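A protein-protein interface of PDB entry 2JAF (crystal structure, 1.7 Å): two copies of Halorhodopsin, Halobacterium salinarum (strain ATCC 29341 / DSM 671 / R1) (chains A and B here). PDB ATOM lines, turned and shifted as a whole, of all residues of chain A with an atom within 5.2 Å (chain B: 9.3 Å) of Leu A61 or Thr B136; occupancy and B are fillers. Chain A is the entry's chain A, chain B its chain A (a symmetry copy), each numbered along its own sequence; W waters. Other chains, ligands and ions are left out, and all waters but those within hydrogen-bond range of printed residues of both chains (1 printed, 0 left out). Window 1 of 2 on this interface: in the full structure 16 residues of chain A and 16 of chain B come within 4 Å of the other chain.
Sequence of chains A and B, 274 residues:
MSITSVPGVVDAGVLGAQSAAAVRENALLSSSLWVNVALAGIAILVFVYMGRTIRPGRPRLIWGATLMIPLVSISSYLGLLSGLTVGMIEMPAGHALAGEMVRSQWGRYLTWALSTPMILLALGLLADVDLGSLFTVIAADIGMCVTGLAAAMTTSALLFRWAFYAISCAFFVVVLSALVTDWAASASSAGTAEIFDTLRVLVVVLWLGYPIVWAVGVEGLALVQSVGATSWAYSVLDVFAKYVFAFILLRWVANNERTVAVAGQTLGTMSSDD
No position is printed for both chains.
Of the 8 pairs that touch across the chains among the printed residues, none has its exchanged pair printed and touching as well.
Among the printed residues, merely in contact across the chains: Arg A60 with Thr B181 (3.9 Å), Leu A61 with Ser B133 (3.6 Å), Leu A61 with Thr B136 (3.7 Å), Met A68 with Thr B136 (3.3 Å), Met A68 with Ala B140 (3.5 Å), Met A68 with Phe B171 (3.9 Å), Leu A121 with Thr B136 (3.6 Å) and Leu A125 with Gly B132 (3.96 Å).
Of the printed residues of chain B, Arg A60 touches Thr B181 (3.9 Å).
Leu A61 touches two residues of chain B.
Of the printed residues of chain B, Met A68 touches Thr B136 (3.3 Å), Ala B140 (3.5 Å) and Phe B171 (3.9 Å).
Of the printed residues of chain A, Ser B133 touches Leu A61 (3.6 Å).
Of chain A, only Leu A61, Met A68 and Leu A121 come within 4 Å of Thr B136.
Asp B141 touches none of the printed residues of chain A.
Printed residues of chain A within 4 Å of Phe B171: Met A68 (3.9 Å).
Trp B183 touches none of the printed residues of chain A.
The nearest residue of chain B that does not touch Leu A61 is Gly B132 (4.03 Å).
Water W1 lies within hydrogen-bond range of the side-chain carboxylate (OD1) of Asp B182, the side-chain hydroxyl (OG1) of Thr B181 and the guanidinium group (NE) of Arg A60.
OG1 of Thr B181 is in hydrogen-bond range of O of Ser B177 (2.6 Å).
The backbone carbonyl oxygen (O) of Gly B132 sits at hydrogen-bond distance from the side-chain hydroxyl (OG1) of Thr B136.
OG of Ser B133 lies within hydrogen-bond range of OD2 of Asp B182.
The side-chain carboxylate (OD1) of Asp B182 sits at hydrogen-bond distance from the side-chain hydroxyl (OG1) of Thr B181, 3.3 Å away.
OG of Ser B133 sits at hydrogen-bond distance from NE1 of Trp B183 (2.8 Å).
NH2 of Arg A58 is in hydrogen-bond range of O of Leu A125 (2.7 Å).
Of the 26 printed residues of chain B, 6 touch a printed residue of chain A.
Printed residues of chain B that touch a printed residue of chain A: Gly B132, Ser B133, Thr B136, Ala B140, Phe B171 and Thr B181.
Hydrophobic or aromatic side chains of chain B that line the printed part of chain A: Ala B140 and Phe B171.
Printed residues of chain A that touch a printed residue of chain B: Arg A60, Leu A61, Met A68, Leu A121 and Leu A125.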
ATOM      1  N   GLY A  57      16.217  -5.688  15.695  1.00  0.00           N
ATOM      2  CA  GLY A  57      16.142  -4.238  15.656  1.00  0.00           C
ATOM      3  C   GLY A  57      15.267  -3.741  14.519  1.00  0.00           C
ATOM      4  O   GLY A  57      14.194  -4.290  14.267  1.00  0.00           O
ATOM      5  N   ARG A  58      15.729  -2.703  13.828  1.00  0.00           N
ATOM      6  CA  ARG A  58      14.992  -2.116  12.712  1.00  0.00           C
ATOM      7  C   ARG A  58      14.682  -3.127  11.602  1.00  0.00           C
ATOM      8  O   ARG A  58      13.537  -3.245  11.163  1.00  0.00           O
ATOM      9  CB  ARG A  58      15.787  -0.947  12.121  1.00  0.00           C
ATOM     10  CG  ARG A  58      16.149   0.139  13.122  1.00  0.00           C
ATOM     11  CD  ARG A  58      14.926   0.908  13.574  1.00  0.00           C
ATOM     12  NE  ARG A  58      14.307   1.641  12.472  1.00  0.00           N
ATOM     13  CZ  ARG A  58      13.248   2.434  12.606  1.00  0.00           C
ATOM     14  NH1 ARG A  58      12.689   2.597  13.800  1.00  0.00           N
ATOM     15  NH2 ARG A  58      12.753   3.071  11.552  1.00  0.00           N
ATOM     16  N   PRO A  59      15.704  -3.866  11.132  1.00  0.00           N
ATOM     17  CA  PRO A  59      15.525  -4.861  10.070  1.00  0.00           C
ATOM     18  C   PRO A  59      14.420  -5.876  10.350  1.00  0.00           C
ATOM     19  O   PRO A  59      13.448  -5.979   9.600  1.00  0.00           O
ATOM     20  CB  PRO A  59      16.898  -5.523   9.985  1.00  0.00           C
ATOM     21  CG  PRO A  59      17.822  -4.413  10.354  1.00  0.00           C
ATOM     22  CD  PRO A  59      17.120  -3.794  11.537  1.00  0.00           C
ATOM     23  N   ARG A  60      14.586  -6.628  11.433  1.00  0.00           N
ATOM     24  CA  ARG A  60      13.624  -7.648  11.829  1.00  0.00           C
ATOM     25  C   ARG A  60      12.221  -7.068  11.983  1.00  0.00           C
ATOM     26  O   ARG A  60      11.231  -7.731  11.679  1.00  0.00           O
ATOM     27  CB  ARG A  60      14.067  -8.288  13.147  1.00  0.00           C
ATOM     28  CG  ARG A  60      13.183  -9.422  13.622  1.00  0.00           C
ATOM     29  CD  ARG A  60      13.588  -9.867  15.017  1.00  0.00           C
ATOM     30  NE  ARG A  60      12.764 -10.967  15.506  1.00  0.00           N
ATOM     31  CZ  ARG A  60      12.761 -12.187  14.979  1.00  0.00           C
ATOM     32  NH1 ARG A  60      13.539 -12.467  13.942  1.00  0.00           N
ATOM     33  NH2 ARG A  60      11.979 -13.126  15.492  1.00  0.00           N
ATOM     34  N   LEU A  61      12.145  -5.830  12.455  1.00  0.00           N
ATOM     35  CA  LEU A  61      10.866  -5.155  12.656  1.00  0.00           C
ATOM     36  C   LEU A  61      10.143  -4.900  11.334  1.00  0.00           C
ATOM     37  O   LEU A  61       8.932  -5.105  11.227  1.00  0.00           O
ATOM     38  CB  LEU A  61      11.085  -3.827  13.383  1.00  0.00           C
ATOM     39  CG  LEU A  61       9.844  -2.972  13.644  1.00  0.00           C
ATOM     40  CD1 LEU A  61       8.830  -3.758  14.466  1.00  0.00           C
ATOM     41  CD2 LEU A  61      10.254  -1.701  14.370  1.00  0.00           C
ATOM     42  N   ILE A  62      10.882  -4.435  10.333  1.00  0.00           N
ATOM     43  CA  ILE A  62      10.287  -4.170   9.030  1.00  0.00           C
ATOM     44  C   ILE A  62       9.933  -5.509   8.390  1.00  0.00           C
ATOM     45  O   ILE A  62       8.973  -5.612   7.628  1.00  0.00           O
ATOM     46  CB  ILE A  62      11.255  -3.382   8.125  1.00  0.00           C
ATOM     47  CG1 ILE A  62      11.551  -2.018   8.755  1.00  0.00           C
ATOM     48  CG2 ILE A  62      10.643  -3.187   6.744  1.00  0.00           C
ATOM     49  CD1 ILE A  62      12.573  -1.193   7.997  1.00  0.00           C
ATOM     50  N   TRP A  63      10.712  -6.535   8.716  1.00  0.00           N
ATOM     51  CA  TRP A  63      10.472  -7.878   8.202  1.00  0.00           C
ATOM     52  C   TRP A  63       9.094  -8.366   8.657  1.00  0.00           C
ATOM     53  O   TRP A  63       8.334  -8.927   7.867  1.00  0.00           O
ATOM     54  CB  TRP A  63      11.545  -8.841   8.713  1.00  0.00           C
ATOM     55  CG  TRP A  63      11.291 -10.273   8.354  1.00  0.00           C
ATOM     56  CD1 TRP A  63      11.188 -10.800   7.098  1.00  0.00           C
ATOM     57  CD2 TRP A  63      11.117 -11.368   9.264  1.00  0.00           C
ATOM     58  NE1 TRP A  63      10.965 -12.155   7.169  1.00  0.00           N
ATOM     59  CE2 TRP A  63      10.917 -12.530   8.487  1.00  0.00           C
ATOM     60  CE3 TRP A  63      11.114 -11.478  10.661  1.00  0.00           C
ATOM     61  CZ2 TRP A  63      10.715 -13.792   9.061  1.00  0.00           C
ATOM     62  CZ3 TRP A  63      10.911 -12.734  11.234  1.00  0.00           C
ATOM     63  CH2 TRP A  63      10.716 -13.873  10.432  1.00  0.00           C
ATOM     64  N   GLY A  64       8.786  -8.150   9.934  1.00  0.00           N
ATOM     65  CA  GLY A  64       7.504  -8.571  10.474  1.00  0.00           C
ATOM     66  C   GLY A  64       6.336  -7.822   9.857  1.00  0.00           C
ATOM     67  O   GLY A  64       5.319  -8.420   9.499  1.00  0.00           O
ATOM     68  N   ALA A  65       6.475  -6.507   9.741  1.00  0.00           N
ATOM     69  CA  ALA A  65       5.431  -5.683   9.153  1.00  0.00           C
ATOM     70  C   ALA A  65       5.196  -6.127   7.715  1.00  0.00           C
ATOM     71  O   ALA A  65       4.060  -6.148   7.231  1.00  0.00           O
ATOM     72  CB  ALA A  65       5.842  -4.218   9.186  1.00  0.00           C
ATOM     73  N   THR A  66       6.278  -6.494   7.038  1.00  0.00           N
ATOM     74  CA  THR A  66       6.187  -6.934   5.652  1.00  0.00           C
ATOM     75  C   THR A  66       5.517  -8.301   5.537  1.00  0.00           C
ATOM     76  O   THR A  66       4.734  -8.535   4.620  1.00  0.00           O
ATOM     77  CB  THR A  66       7.584  -6.990   5.002  1.00  0.00           C
ATOM     78  OG1 THR A  66       8.192  -5.692   5.080  1.00  0.00           O
ATOM     79  CG2 THR A  66       7.477  -7.397   3.542  1.00  0.00           C
ATOM     80  N   MET A  68       3.190  -9.502   7.247  1.00  0.00           N
ATOM     81  CA  MET A  68       1.750  -9.398   7.402  1.00  0.00           C
ATOM     82  C   MET A  68       0.985  -8.875   6.207  1.00  0.00           C
ATOM     83  O   MET A  68      -0.230  -9.028   6.147  1.00  0.00           O
ATOM     84  CB  MET A  68       1.424  -8.556   8.615  1.00  0.00           C
ATOM     85  CG  MET A  68       1.653  -9.313   9.899  1.00  0.00           C
ATOM     86  SD  MET A  68       0.887  -8.432  11.212  1.00  0.00           S
ATOM     87  CE  MET A  68       2.223  -7.336  11.651  1.00  0.00           C
ATOM     88  N   LEU A 121       3.048   1.336   7.014  1.00  0.00           N
ATOM     89  CA  LEU A 121       3.849   1.144   8.217  1.00  0.00           C
ATOM     90  C   LEU A 121       5.245   0.674   7.807  1.00  0.00           C
ATOM     91  O   LEU A 121       6.255   1.193   8.283  1.00  0.00           O
ATOM     92  CB  LEU A 121       3.199   0.102   9.135  1.00  0.00           C
ATOM     93  CG  LEU A 121       4.032  -0.296  10.360  1.00  0.00           C
ATOM     94  CD1 LEU A 121       4.328   0.935  11.213  1.00  0.00           C
ATOM     95  CD2 LEU A 121       3.288  -1.346  11.161  1.00  0.00           C
ATOM     96  N   LEU A 125       8.573   2.864   8.467  1.00  0.00           N
ATOM     97  CA  LEU A 125       9.686   2.408   9.290  1.00  0.00           C
ATOM     98  C   LEU A 125      10.969   2.512   8.467  1.00  0.00           C
ATOM     99  O   LEU A 125      11.980   3.026   8.935  1.00  0.00           O
ATOM    100  CB  LEU A 125       9.458   0.961   9.738  1.00  0.00           C
ATOM    101  CG  LEU A 125       8.285   0.724  10.694  1.00  0.00           C
ATOM    102  CD1 LEU A 125       8.075  -0.764  10.914  1.00  0.00           C
ATOM    103  CD2 LEU A 125       8.565   1.426  12.017  1.00  0.00           C
ATOM    104  N   LEU B 120      -1.800  -5.094  25.445  1.00  0.00           N
ATOM    105  CA  LEU B 120      -0.488  -4.964  24.813  1.00  0.00           C
ATOM    106  C   LEU B 120       0.083  -3.556  24.993  1.00  0.00           C
ATOM    107  O   LEU B 120       1.294  -3.376  25.105  1.00  0.00           O
ATOM    108  CB  LEU B 120      -0.590  -5.322  23.324  1.00  0.00           C
ATOM    109  CG  LEU B 120      -1.005  -6.786  23.077  1.00  0.00           C
ATOM    110  CD1 LEU B 120      -1.303  -7.026  21.599  1.00  0.00           C
ATOM    111  CD2 LEU B 120       0.112  -7.712  23.554  1.00  0.00           C
ATOM    112  N   VAL B 129       8.898  -0.177  24.948  1.00  0.00           N
ATOM    113  CA  VAL B 129       9.325  -0.662  23.640  1.00  0.00           C
ATOM    114  C   VAL B 129       9.257   0.429  22.578  1.00  0.00           C
ATOM    115  O   VAL B 129       8.722   1.508  22.817  1.00  0.00           O
ATOM    116  CB  VAL B 129       8.442  -1.845  23.180  1.00  0.00           C
ATOM    117  CG1 VAL B 129       8.460  -2.947  24.232  1.00  0.00           C
ATOM    118  CG2 VAL B 129       7.019  -1.368  22.936  1.00  0.00           C
ATOM    119  N   ASP B 130       9.803   0.142  21.401  1.00  0.00           N
ATOM    120  CA  ASP B 130       9.781   1.106  20.305  1.00  0.00           C
ATOM    121  C   ASP B 130       8.349   1.299  19.833  1.00  0.00           C
ATOM    122  O   ASP B 130       7.569   0.347  19.787  1.00  0.00           O
ATOM    123  CB  ASP B 130      10.635   0.609  19.135  1.00  0.00           C
ATOM    124  CG  ASP B 130      12.112   0.557  19.469  1.00  0.00           C
ATOM    125  OD1 ASP B 130      12.682   1.616  19.809  1.00  0.00           O
ATOM    126  OD2 ASP B 130      12.703  -0.541  19.387  1.00  0.00           O
ATOM    127  N   LEU B 131       8.002   2.536  19.488  1.00  0.00           N
ATOM    128  CA  LEU B 131       6.660   2.847  19.014  1.00  0.00           C
ATOM    129  C   LEU B 131       6.342   2.029  17.766  1.00  0.00           C
ATOM    130  O   LEU B 131       5.205   1.599  17.567  1.00  0.00           O
ATOM    131  CB  LEU B 131       6.537   4.339  18.688  1.00  0.00           C
ATOM    132  CG  LEU B 131       6.832   5.366  19.786  1.00  0.00           C
ATOM    133  CD1 LEU B 131       6.039   5.008  21.038  1.00  0.00           C
ATOM    134  CD2 LEU B 131       8.329   5.400  20.088  1.00  0.00           C
ATOM    135  N   GLY B 132       7.355   1.822  16.929  1.00  0.00           N
ATOM    136  CA  GLY B 132       7.170   1.060  15.707  1.00  0.00           C
ATOM    137  C   GLY B 132       6.809  -0.384  15.986  1.00  0.00           C
ATOM    138  O   GLY B 132       5.962  -0.970  15.307  1.00  0.00           O
ATOM    139  N   SER B 133       7.463  -0.967  16.987  1.00  0.00           N
ATOM    140  CA  SER B 133       7.201  -2.347  17.368  1.00  0.00           C
ATOM    141  C   SER B 133       5.781  -2.441  17.924  1.00  0.00           C
ATOM    142  O   SER B 133       5.022  -3.342  17.573  1.00  0.00           O
ATOM    143  CB  SER B 133       8.211  -2.800  18.426  1.00  0.00           C
ATOM    144  OG  SER B 133       8.021  -4.161  18.770  1.00  0.00           O
ATOM    145  N   LEU B 134       5.422  -1.496  18.786  1.00  0.00           N
ATOM    146  CA  LEU B 134       4.091  -1.483  19.378  1.00  0.00           C
ATOM    147  C   LEU B 134       3.040  -1.450  18.276  1.00  0.00           C
ATOM    148  O   LEU B 134       2.042  -2.169  18.328  1.00  0.00           O
ATOM    149  CB  LEU B 134       3.931  -0.265  20.289  1.00  0.00           C
ATOM    150  CG  LEU B 134       2.584  -0.092  20.994  1.00  0.00           C
ATOM    151  CD1 LEU B 134       2.336  -1.254  21.945  1.00  0.00           C
ATOM    152  CD2 LEU B 134       2.582   1.227  21.748  1.00  0.00           C
ATOM    153  N   PHE B 135       3.283  -0.607  17.278  1.00  0.00           N
ATOM    154  CA  PHE B 135       2.387  -0.451  16.137  1.00  0.00           C
ATOM    155  C   PHE B 135       2.151  -1.775  15.413  1.00  0.00           C
ATOM    156  O   PHE B 135       1.013  -2.172  15.153  1.00  0.00           O
ATOM    157  CB  PHE B 135       2.987   0.548  15.138  1.00  0.00           C
ATOM    158  CG  PHE B 135       2.348   1.909  15.167  1.00  0.00           C
ATOM    159  CD1 PHE B 135       0.982   2.057  14.939  1.00  0.00           C
ATOM    160  CD2 PHE B 135       3.119   3.050  15.380  1.00  0.00           C
ATOM    161  CE1 PHE B 135       0.393   3.323  14.918  1.00  0.00           C
ATOM    162  CE2 PHE B 135       2.541   4.320  15.362  1.00  0.00           C
ATOM    163  CZ  PHE B 135       1.175   4.456  15.130  1.00  0.00           C
ATOM    164  N   THR B 136       3.244  -2.447  15.080  1.00  0.00           N
ATOM    165  CA  THR B 136       3.181  -3.709  14.361  1.00  0.00           C
ATOM    166  C   THR B 136       2.436  -4.775  15.144  1.00  0.00           C
ATOM    167  O   THR B 136       1.655  -5.546  14.580  1.00  0.00           O
ATOM    168  CB  THR B 136       4.593  -4.225  14.052  1.00  0.00           C
ATOM    169  OG1 THR B 136       5.343  -3.196  13.394  1.00  0.00           O
ATOM    170  CG2 THR B 136       4.524  -5.439  13.146  1.00  0.00           C
ATOM    171  N   VAL B 137       2.673  -4.803  16.449  1.00  0.00           N
ATOM    172  CA  VAL B 137       2.041  -5.789  17.314  1.00  0.00           C
ATOM    173  C   VAL B 137       0.539  -5.586  17.442  1.00  0.00           C
ATOM    174  O   VAL B 137      -0.227  -6.554  17.427  1.00  0.00           O
ATOM    175  CB  VAL B 137       2.712  -5.788  18.708  1.00  0.00           C
ATOM    176  CG1 VAL B 137       1.980  -6.729  19.651  1.00  0.00           C
ATOM    177  CG2 VAL B 137       4.160  -6.212  18.569  1.00  0.00           C
ATOM    178  N   ILE B 138       0.106  -4.334  17.549  1.00  0.00           N
ATOM    179  CA  ILE B 138      -1.318  -4.048  17.670  1.00  0.00           C
ATOM    180  C   ILE B 138      -2.040  -4.409  16.377  1.00  0.00           C
ATOM    181  O   ILE B 138      -3.163  -4.919  16.396  1.00  0.00           O
ATOM    182  CB  ILE B 138      -1.551  -2.560  18.021  1.00  0.00           C
ATOM    183  CG1 ILE B 138      -0.982  -2.283  19.421  1.00  0.00           C
ATOM    184  CG2 ILE B 138      -3.043  -2.227  17.974  1.00  0.00           C
ATOM    185  CD1 ILE B 138      -1.180  -0.867  19.916  1.00  0.00           C
ATOM    186  N   ALA B 139      -1.385  -4.155  15.250  1.00  0.00           N
ATOM    187  CA  ALA B 139      -1.973  -4.471  13.959  1.00  0.00           C
ATOM    188  C   ALA B 139      -2.132  -5.981  13.840  1.00  0.00           C
ATOM    189  O   ALA B 139      -3.160  -6.468  13.373  1.00  0.00           O
ATOM    190  CB  ALA B 139      -1.089  -3.948  12.839  1.00  0.00           C
ATOM    191  N   ALA B 140      -1.111  -6.716  14.271  1.00  0.00           N
ATOM    192  CA  ALA B 140      -1.150  -8.172  14.200  1.00  0.00           C
ATOM    193  C   ALA B 140      -2.250  -8.685  15.106  1.00  0.00           C
ATOM    194  O   ALA B 140      -2.956  -9.648  14.783  1.00  0.00           O
ATOM    195  CB  ALA B 140       0.199  -8.757  14.626  1.00  0.00           C
ATOM    196  N   ASP B 141      -2.396  -8.028  16.250  1.00  0.00           N
ATOM    197  CA  ASP B 141      -3.403  -8.409  17.221  1.00  0.00           C
ATOM    198  C   ASP B 141      -4.796  -8.188  16.648  1.00  0.00           C
ATOM    199  O   ASP B 141      -5.679  -9.029  16.792  1.00  0.00           O
ATOM    200  CB  ASP B 141      -3.222  -7.589  18.498  1.00  0.00           C
ATOM    201  CG  ASP B 141      -4.130  -8.051  19.615  1.00  0.00           C
ATOM    202  OD1 ASP B 141      -3.829  -9.088  20.246  1.00  0.00           O
ATOM    203  OD2 ASP B 141      -5.153  -7.381  19.847  1.00  0.00           O
ATOM    204  N   ILE B 142      -4.992  -7.047  15.990  1.00  0.00           N
ATOM    205  CA  ILE B 142      -6.288  -6.750  15.397  1.00  0.00           C
ATOM    206  C   ILE B 142      -6.598  -7.791  14.325  1.00  0.00           C
ATOM    207  O   ILE B 142      -7.732  -8.251  14.212  1.00  0.00           O
ATOM    208  CB  ILE B 142      -6.305  -5.317  14.805  1.00  0.00           C
ATOM    209  CG1 ILE B 142      -6.247  -4.303  15.960  1.00  0.00           C
ATOM    210  CG2 ILE B 142      -7.569  -5.095  13.984  1.00  0.00           C
ATOM    211  CD1 ILE B 142      -6.081  -2.853  15.521  1.00  0.00           C
ATOM    212  N   GLY B 143      -5.584  -8.172  13.555  1.00  0.00           N
ATOM    213  CA  GLY B 143      -5.775  -9.181  12.524  1.00  0.00           C
ATOM    214  C   GLY B 143      -6.211 -10.508  13.124  1.00  0.00           C
ATOM    215  O   GLY B 143      -7.087 -11.191  12.586  1.00  0.00           O
ATOM    216  N   MET B 144      -5.600 -10.880  14.248  1.00  0.00           N
ATOM    217  CA  MET B 144      -5.943 -12.133  14.918  1.00  0.00           C
ATOM    218  C   MET B 144      -7.412 -12.102  15.324  1.00  0.00           C
ATOM    219  O   MET B 144      -8.160 -13.059  15.103  1.00  0.00           O
ATOM    220  CB  MET B 144      -5.052 -12.329  16.163  1.00  0.00           C
ATOM    221  CG  MET B 144      -5.435 -13.503  17.072  1.00  0.00           C
ATOM    222  SD  MET B 144      -4.497 -13.480  18.633  1.00  0.00           S
ATOM    223  CE  MET B 144      -5.435 -12.258  19.538  1.00  0.00           C
ATOM    224  N   PHE B 171      -1.369 -14.737  13.009  1.00  0.00           N
ATOM    225  CA  PHE B 171      -1.252 -13.392  13.559  1.00  0.00           C
ATOM    226  C   PHE B 171      -0.844 -13.476  15.026  1.00  0.00           C
ATOM    227  O   PHE B 171      -0.048 -12.665  15.514  1.00  0.00           O
ATOM    228  CB  PHE B 171      -2.578 -12.639  13.443  1.00  0.00           C
ATOM    229  CG  PHE B 171      -2.835 -12.068  12.076  1.00  0.00           C
ATOM    230  CD1 PHE B 171      -2.006 -11.081  11.554  1.00  0.00           C
ATOM    231  CD2 PHE B 171      -3.929 -12.493  11.325  1.00  0.00           C
ATOM    232  CE1 PHE B 171      -2.262 -10.517  10.298  1.00  0.00           C
ATOM    233  CE2 PHE B 171      -4.192 -11.934  10.072  1.00  0.00           C
ATOM    234  CZ  PHE B 171      -3.358 -10.946   9.562  1.00  0.00           C
ATOM    235  N   VAL B 174       2.744 -13.738  15.447  1.00  0.00           N
ATOM    236  CA  VAL B 174       3.450 -12.471  15.254  1.00  0.00           C
ATOM    237  C   VAL B 174       3.458 -11.721  16.580  1.00  0.00           C
ATOM    238  O   VAL B 174       4.473 -11.137  16.972  1.00  0.00           O
ATOM    239  CB  VAL B 174       2.768 -11.587  14.197  1.00  0.00           C
ATOM    240  CG1 VAL B 174       3.478 -10.237  14.120  1.00  0.00           C
ATOM    241  CG2 VAL B 174       2.796 -12.278  12.839  1.00  0.00           C
ATOM    242  N   VAL B 175       2.322 -11.740  17.270  1.00  0.00           N
ATOM    243  CA  VAL B 175       2.205 -11.083  18.568  1.00  0.00           C
ATOM    244  C   VAL B 175       3.173 -11.706  19.569  1.00  0.00           C
ATOM    245  O   VAL B 175       3.921 -10.999  20.254  1.00  0.00           O
ATOM    246  CB  VAL B 175       0.770 -11.206  19.141  1.00  0.00           C
ATOM    247  CG1 VAL B 175       0.738 -10.732  20.590  1.00  0.00           C
ATOM    248  CG2 VAL B 175      -0.201 -10.386  18.294  1.00  0.00           C
ATOM    249  N   LEU B 176       3.161 -13.032  19.658  1.00  0.00           N
ATOM    250  CA  LEU B 176       4.039 -13.717  20.601  1.00  0.00           C
ATOM    251  C   LEU B 176       5.516 -13.507  20.303  1.00  0.00           C
ATOM    252  O   LEU B 176       6.333 -13.438  21.226  1.00  0.00           O
ATOM    253  CB  LEU B 176       3.722 -15.216  20.629  1.00  0.00           C
ATOM    254  CG  LEU B 176       2.336 -15.566  21.176  1.00  0.00           C
ATOM    255  CD1 LEU B 176       2.078 -17.054  21.040  1.00  0.00           C
ATOM    256  CD2 LEU B 176       2.247 -15.136  22.626  1.00  0.00           C
ATOM    257  N   SER B 177       5.860 -13.393  19.023  1.00  0.00           N
ATOM    258  CA  SER B 177       7.253 -13.209  18.625  1.00  0.00           C
ATOM    259  C   SER B 177       7.858 -11.962  19.260  1.00  0.00           C
ATOM    260  O   SER B 177       9.033 -11.949  19.616  1.00  0.00           O
ATOM    261  CB  SER B 177       7.379 -13.116  17.094  1.00  0.00           C
ATOM    262  OG  SER B 177       6.893 -11.877  16.598  1.00  0.00           O
ATOM    263  N   ALA B 178       7.058 -10.911  19.393  1.00  0.00           N
ATOM    264  CA  ALA B 178       7.544  -9.677  19.992  1.00  0.00           C
ATOM    265  C   ALA B 178       7.867  -9.912  21.467  1.00  0.00           C
ATOM    266  O   ALA B 178       8.907  -9.466  21.966  1.00  0.00           O
ATOM    267  CB  ALA B 178       6.495  -8.576  19.847  1.00  0.00           C
ATOM    268  N   THR B 181      11.145 -11.669  21.867  1.00  0.00           N
ATOM    269  CA  THR B 181      12.336 -11.020  21.335  1.00  0.00           C
ATOM    270  C   THR B 181      12.578  -9.572  21.763  1.00  0.00           C
ATOM    271  O   THR B 181      12.991  -9.326  22.897  1.00  0.00           O
ATOM    272  CB  THR B 181      12.389 -11.118  19.780  1.00  0.00           C
ATOM    273  OG1 THR B 181      11.206 -10.545  19.206  1.00  0.00           O
ATOM    274  CG2 THR B 181      12.502 -12.572  19.348  1.00  0.00           C
ATOM    275  N   ASP B 182      12.319  -8.614  20.874  1.00  0.00           N
ATOM    276  CA  ASP B 182      12.587  -7.210  21.180  1.00  0.00           C
ATOM    277  C   ASP B 182      11.887  -6.592  22.390  1.00  0.00           C
ATOM    278  O   ASP B 182      12.456  -5.722  23.044  1.00  0.00           O
ATOM    279  CB  ASP B 182      12.348  -6.343  19.937  1.00  0.00           C
ATOM    280  CG  ASP B 182      10.907  -6.330  19.504  1.00  0.00           C
ATOM    281  OD1 ASP B 182      10.317  -7.419  19.364  1.00  0.00           O
ATOM    282  OD2 ASP B 182      10.368  -5.225  19.291  1.00  0.00           O
ATOM    283  N   TRP B 183      10.670  -7.026  22.704  1.00  0.00           N
ATOM    284  CA  TRP B 183       9.976  -6.476  23.865  1.00  0.00           C
ATOM    285  C   TRP B 183      10.689  -6.886  25.153  1.00  0.00           C
ATOM    286  O   TRP B 183      10.674  -6.151  26.142  1.00  0.00           O
ATOM    287  CB  TRP B 183       8.516  -6.946  23.900  1.00  0.00           C
ATOM    288  CG  TRP B 183       7.621  -6.162  22.982  1.00  0.00           C
ATOM    289  CD1 TRP B 183       7.938  -5.678  21.743  1.00  0.00           C
ATOM    290  CD2 TRP B 183       6.250  -5.812  23.210  1.00  0.00           C
ATOM    291  NE1 TRP B 183       6.851  -5.049  21.189  1.00  0.00           N
ATOM    292  CE2 TRP B 183       5.801  -5.117  22.064  1.00  0.00           C
ATOM    293  CE3 TRP B 183       5.358  -6.020  24.268  1.00  0.00           C
ATOM    294  CZ2 TRP B 183       4.497  -4.627  21.948  1.00  0.00           C
ATOM    295  CZ3 TRP B 183       4.060  -5.532  24.153  1.00  0.00           C
ATOM    296  CH2 TRP B 183       3.643  -4.844  23.002  1.00  0.00           C
HETATM  297  O   HOH W   1      11.046  -8.642  16.946  1.00  0.00           O
